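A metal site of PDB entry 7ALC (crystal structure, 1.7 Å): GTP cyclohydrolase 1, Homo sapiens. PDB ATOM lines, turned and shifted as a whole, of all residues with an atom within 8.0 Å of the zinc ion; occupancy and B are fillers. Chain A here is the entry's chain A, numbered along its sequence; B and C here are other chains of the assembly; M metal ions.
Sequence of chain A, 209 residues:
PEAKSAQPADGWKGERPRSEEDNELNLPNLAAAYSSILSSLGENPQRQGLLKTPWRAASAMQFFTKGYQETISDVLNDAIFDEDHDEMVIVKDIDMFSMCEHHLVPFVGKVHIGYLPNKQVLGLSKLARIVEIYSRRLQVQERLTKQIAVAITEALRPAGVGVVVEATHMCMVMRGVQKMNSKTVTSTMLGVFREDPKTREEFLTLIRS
A ring nitrogen (ND1) of His 103 binds the zinc ion (2.1 Å).
SG of Cys 100 is bound to the zinc ion.
SG of Cys 171 is bound to the zinc ion (2.3 Å).
The zinc ion has three donor atoms within binding distance.
N of Cys 100 lies within hydrogen-bond range of O of Val 105 (3.0 Å).
The side-chain sulfur of Cys 100 lies close to the backbone NH of His 102, at 3.3 Å.
Three residues have an atom within 4 Å of the zinc ion: Cys 100, His 103 and Cys 171.
The nearest printed residue that does not touch the zinc ion is His 102 (4.3 Å).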
ATOM      1  N   MET A  99     -11.299  -9.856  13.893  1.00  0.00           N
ATOM      2  CA  MET A  99     -10.968 -11.260  13.938  1.00  0.00           C
ATOM      3  C   MET A  99     -12.206 -12.041  13.639  1.00  0.00           C
ATOM      4  O   MET A  99     -13.230 -11.845  14.279  1.00  0.00           O
ATOM      5  CB  MET A  99     -10.478 -11.631  15.348  1.00  0.00           C
ATOM      6  CG  MET A  99      -9.025 -11.846  15.412  1.00  0.00           C
ATOM      7  SD  MET A  99      -8.384 -13.415  14.809  1.00  0.00           S
ATOM      8  CE  MET A  99      -6.724 -13.118  15.247  1.00  0.00           C
ATOM      9  N   CYS A 100     -12.133 -12.932  12.681  1.00  0.00           N
ATOM     10  CA  CYS A 100     -13.246 -13.781  12.315  1.00  0.00           C
ATOM     11  C   CYS A 100     -13.576 -14.712  13.537  1.00  0.00           C
ATOM     12  O   CYS A 100     -12.658 -15.363  14.048  1.00  0.00           O
ATOM     13  CB  CYS A 100     -12.823 -14.595  11.098  1.00  0.00           C
ATOM     14  SG  CYS A 100     -13.636 -16.191  10.934  1.00  0.00           S
ATOM     15  N   GLU A 101     -14.826 -14.709  14.026  1.00  0.00           N
ATOM     16  CA  GLU A 101     -15.163 -15.571  15.162  1.00  0.00           C
ATOM     17  C   GLU A 101     -15.263 -17.037  14.777  1.00  0.00           C
ATOM     18  O   GLU A 101     -15.174 -17.892  15.657  1.00  0.00           O
ATOM     19  CB  GLU A 101     -16.455 -15.127  15.844  1.00  0.00           C
ATOM     20  CG  GLU A 101     -17.701 -15.365  15.033  1.00  0.00           C
ATOM     21  CD  GLU A 101     -18.939 -14.777  15.674  1.00  0.00           C
ATOM     22  OE1 GLU A 101     -20.045 -15.271  15.384  1.00  0.00           O
ATOM     23  OE2 GLU A 101     -18.806 -13.823  16.483  1.00  0.00           O
ATOM     24  N   HIS A 102     -15.460 -17.344  13.495  1.00  0.00           N
ATOM     25  CA  HIS A 102     -15.573 -18.730  13.046  1.00  0.00           C
ATOM     26  C   HIS A 102     -14.242 -19.433  12.986  1.00  0.00           C
ATOM     27  O   HIS A 102     -14.173 -20.598  13.333  1.00  0.00           O
ATOM     28  CB  HIS A 102     -16.280 -18.796  11.698  1.00  0.00           C
ATOM     29  CG  HIS A 102     -17.680 -18.291  11.734  1.00  0.00           C
ATOM     30  ND1 HIS A 102     -18.267 -17.722  10.630  1.00  0.00           N
ATOM     31  CD2 HIS A 102     -18.576 -18.298  12.759  1.00  0.00           C
ATOM     32  CE1 HIS A 102     -19.494 -17.396  11.002  1.00  0.00           C
ATOM     33  NE2 HIS A 102     -19.727 -17.715  12.276  1.00  0.00           N
ATOM     34  N   HIS A 103     -13.164 -18.748  12.549  1.00  0.00           N
ATOM     35  CA  HIS A 103     -11.866 -19.405  12.393  1.00  0.00           C
ATOM     36  C   HIS A 103     -10.729 -18.810  13.211  1.00  0.00           C
ATOM     37  O   HIS A 103      -9.638 -19.364  13.196  1.00  0.00           O
ATOM     38  CB  HIS A 103     -11.455 -19.384  10.914  1.00  0.00           C
ATOM     39  CG  HIS A 103     -12.475 -19.991  10.003  1.00  0.00           C
ATOM     40  ND1 HIS A 103     -13.385 -19.196   9.331  1.00  0.00           N
ATOM     41  CD2 HIS A 103     -12.705 -21.285   9.693  1.00  0.00           C
ATOM     42  CE1 HIS A 103     -14.155 -20.035   8.650  1.00  0.00           C
ATOM     43  NE2 HIS A 103     -13.786 -21.304   8.845  1.00  0.00           N
ATOM     44  N   LEU A 104     -10.946 -17.668  13.878  1.00  0.00           N
ATOM     45  CA  LEU A 104      -9.926 -16.958  14.636  1.00  0.00           C
ATOM     46  C   LEU A 104      -8.760 -16.491  13.761  1.00  0.00           C
ATOM     47  O   LEU A 104      -7.612 -16.561  14.150  1.00  0.00           O
ATOM     48  CB  LEU A 104      -9.431 -17.751  15.866  1.00  0.00           C
ATOM     49  CG  LEU A 104     -10.532 -18.138  16.866  1.00  0.00           C
ATOM     50  CD1 LEU A 104      -9.928 -18.824  18.102  1.00  0.00           C
ATOM     51  CD2 LEU A 104     -11.379 -16.929  17.286  1.00  0.00           C
ATOM     52  N   VAL A 105      -9.091 -16.039  12.555  1.00  0.00           N
ATOM     53  CA  VAL A 105      -8.130 -15.516  11.586  1.00  0.00           C
ATOM     54  C   VAL A 105      -8.564 -14.079  11.274  1.00  0.00           C
ATOM     55  O   VAL A 105      -9.757 -13.839  11.118  1.00  0.00           O
ATOM     56  CB  VAL A 105      -8.113 -16.382  10.300  1.00  0.00           C
ATOM     57  CG1 VAL A 105      -7.090 -15.853   9.321  1.00  0.00           C
ATOM     58  CG2 VAL A 105      -7.809 -17.850  10.621  1.00  0.00           C
ATOM     59  N   PRO A 106      -7.643 -13.113  11.210  1.00  0.00           N
ATOM     60  CA  PRO A 106      -8.059 -11.736  10.964  1.00  0.00           C
ATOM     61  C   PRO A 106      -8.775 -11.501   9.638  1.00  0.00           C
ATOM     62  O   PRO A 106      -8.553 -12.199   8.642  1.00  0.00           O
ATOM     63  CB  PRO A 106      -6.752 -10.934  11.013  1.00  0.00           C
ATOM     64  CG  PRO A 106      -5.773 -11.789  11.730  1.00  0.00           C
ATOM     65  CD  PRO A 106      -6.168 -13.207  11.393  1.00  0.00           C
ATOM     66  N   PHE A 107      -9.658 -10.513   9.651  1.00  0.00           N
ATOM     67  CA  PHE A 107     -10.255  -9.975   8.445  1.00  0.00           C
ATOM     68  C   PHE A 107      -9.993  -8.477   8.529  1.00  0.00           C
ATOM     69  O   PHE A 107     -10.150  -7.862   9.598  1.00  0.00           O
ATOM     70  CB  PHE A 107     -11.728 -10.374   8.217  1.00  0.00           C
ATOM     71  CG  PHE A 107     -12.798  -9.855   9.132  1.00  0.00           C
ATOM     72  CD1 PHE A 107     -13.548  -8.742   8.801  1.00  0.00           C
ATOM     73  CD2 PHE A 107     -13.176 -10.582  10.248  1.00  0.00           C
ATOM     74  CE1 PHE A 107     -14.605  -8.322   9.599  1.00  0.00           C
ATOM     75  CE2 PHE A 107     -14.220 -10.156  11.056  1.00  0.00           C
ATOM     76  CZ  PHE A 107     -14.936  -9.030  10.726  1.00  0.00           C
ATOM     77  N   GLN A 139     -15.723 -11.428  15.568  1.00  0.00           N
ATOM     78  CA  GLN A 139     -16.812 -10.895  14.830  1.00  0.00           C
ATOM     79  C   GLN A 139     -17.241 -11.655  13.588  1.00  0.00           C
ATOM     80  O   GLN A 139     -16.573 -12.581  13.141  1.00  0.00           O
ATOM     81  CB  GLN A 139     -16.377  -9.466  14.395  1.00  0.00           C
ATOM     82  CG  GLN A 139     -16.573  -8.375  15.449  1.00  0.00           C
ATOM     83  CD  GLN A 139     -18.019  -7.994  15.637  1.00  0.00           C
ATOM     84  OE1 GLN A 139     -18.945  -8.654  15.172  1.00  0.00           O
ATOM     85  NE2 GLN A 139     -18.260  -6.910  16.340  1.00  0.00           N
ATOM     86  N   VAL A 140     -18.360 -11.228  13.003  1.00  0.00           N
ATOM     87  CA  VAL A 140     -18.818 -11.540  11.664  1.00  0.00           C
ATOM     88  C   VAL A 140     -19.014 -10.140  11.035  1.00  0.00           C
ATOM     89  O   VAL A 140     -19.445  -9.204  11.720  1.00  0.00           O
ATOM     90  CB  VAL A 140     -20.043 -12.460  11.535  1.00  0.00           C
ATOM     91  CG1 VAL A 140     -19.741 -13.844  12.133  1.00  0.00           C
ATOM     92  CG2 VAL A 140     -21.259 -11.867  12.177  1.00  0.00           C
ATOM     93  N   HIS A 169     -10.947 -11.480   3.945  1.00  0.00           N
ATOM     94  CA  HIS A 169     -10.998 -12.468   5.008  1.00  0.00           C
ATOM     95  C   HIS A 169      -9.837 -13.430   4.822  1.00  0.00           C
ATOM     96  O   HIS A 169      -9.814 -14.141   3.828  1.00  0.00           O
ATOM     97  CB  HIS A 169     -12.355 -13.178   4.986  1.00  0.00           C
ATOM     98  CG  HIS A 169     -13.487 -12.303   5.446  1.00  0.00           C
ATOM     99  ND1 HIS A 169     -14.158 -12.551   6.631  1.00  0.00           N
ATOM    100  CD2 HIS A 169     -13.990 -11.163   4.894  1.00  0.00           C
ATOM    101  CE1 HIS A 169     -15.061 -11.575   6.745  1.00  0.00           C
ATOM    102  NE2 HIS A 169     -14.989 -10.718   5.732  1.00  0.00           N
ATOM    103  N   MET A 170      -8.821 -13.390   5.732  1.00  0.00           N
ATOM    104  CA  MET A 170      -7.616 -14.223   5.615  1.00  0.00           C
ATOM    105  C   MET A 170      -7.878 -15.701   5.693  1.00  0.00           C
ATOM    106  O   MET A 170      -7.064 -16.486   5.214  1.00  0.00           O
ATOM    107  CB  MET A 170      -6.534 -13.845   6.640  1.00  0.00           C
ATOM    108  CG  MET A 170      -6.130 -12.384   6.618  1.00  0.00           C
ATOM    109  SD  MET A 170      -5.296 -11.927   5.095  1.00  0.00           S
ATOM    110  CE  MET A 170      -5.892 -10.324   4.908  1.00  0.00           C
ATOM    111  N   CYS A 171      -8.987 -16.114   6.331  1.00  0.00           N
ATOM    112  CA  CYS A 171      -9.327 -17.533   6.435  1.00  0.00           C
ATOM    113  C   CYS A 171      -9.774 -18.094   5.067  1.00  0.00           C
ATOM    114  O   CYS A 171      -9.746 -19.317   4.899  1.00  0.00           O
ATOM    115  CB  CYS A 171     -10.378 -17.763   7.506  1.00  0.00           C
ATOM    116  SG  CYS A 171     -11.953 -16.912   7.179  1.00  0.00           S
ATOM    117  N   MET A 172     -10.162 -17.233   4.112  1.00  0.00           N
ATOM    118  CA  MET A 172     -10.574 -17.608   2.767  1.00  0.00           C
ATOM    119  C   MET A 172      -9.300 -17.853   1.959  1.00  0.00           C
ATOM    120  O   MET A 172      -8.926 -19.001   1.721  1.00  0.00           O
ATOM    121  CB  MET A 172     -11.374 -16.451   2.140  1.00  0.00           C
ATOM    122  CG  MET A 172     -12.033 -16.787   0.802  1.00  0.00           C
ATOM    123  SD  MET A 172     -13.094 -15.433   0.172  1.00  0.00           S
ATOM    124  CE  MET A 172     -13.862 -16.254  -1.219  1.00  0.00           C
ATOM    125  N   LEU B 124     -18.449 -17.923   3.208  1.00  0.00           N
ATOM    126  CA  LEU B 124     -17.480 -17.653   2.141  1.00  0.00           C
ATOM    127  C   LEU B 124     -16.996 -18.920   1.442  1.00  0.00           C
ATOM    128  O   LEU B 124     -16.931 -18.915   0.218  1.00  0.00           O
ATOM    129  CB  LEU B 124     -16.268 -16.882   2.671  1.00  0.00           C
ATOM    130  CG  LEU B 124     -16.283 -15.355   2.570  1.00  0.00           C
ATOM    131  CD1 LEU B 124     -17.485 -14.757   3.252  1.00  0.00           C
ATOM    132  CD2 LEU B 124     -15.055 -14.792   3.234  1.00  0.00           C
ATOM    133  N   ARG C  56     -13.104 -25.352  13.858  1.00  0.00           N
ATOM    134  CA  ARG C  56     -12.792 -24.581  12.636  1.00  0.00           C
ATOM    135  C   ARG C  56     -11.414 -23.925  12.763  1.00  0.00           C
ATOM    136  O   ARG C  56     -10.612 -23.974  11.816  1.00  0.00           O
ATOM    137  CB  ARG C  56     -13.889 -23.511  12.377  1.00  0.00           C
ATOM    138  CG  ARG C  56     -15.233 -24.071  11.935  1.00  0.00           C
ATOM    139  CD  ARG C  56     -16.237 -22.951  11.659  1.00  0.00           C
ATOM    140  NE  ARG C  56     -16.531 -22.157  12.873  1.00  0.00           N
ATOM    141  CZ  ARG C  56     -17.750 -21.847  13.284  1.00  0.00           C
ATOM    142  NH1 ARG C  56     -17.926 -21.148  14.410  1.00  0.00           N
ATOM    143  NH2 ARG C  56     -18.822 -22.229  12.590  1.00  0.00           N
ATOM    144  N   ALA C  60      -8.117 -24.840  10.444  1.00  0.00           N
ATOM    145  CA  ALA C  60      -7.470 -23.771   9.700  1.00  0.00           C
ATOM    146  C   ALA C  60      -5.983 -23.754  10.030  1.00  0.00           C
ATOM    147  O   ALA C  60      -5.176 -23.743   9.107  1.00  0.00           O
ATOM    148  CB  ALA C  60      -8.103 -22.433  10.046  1.00  0.00           C
HETATM  149 ZN    ZN M   1     -13.302 -17.112   9.029  1.00  0.00          ZN
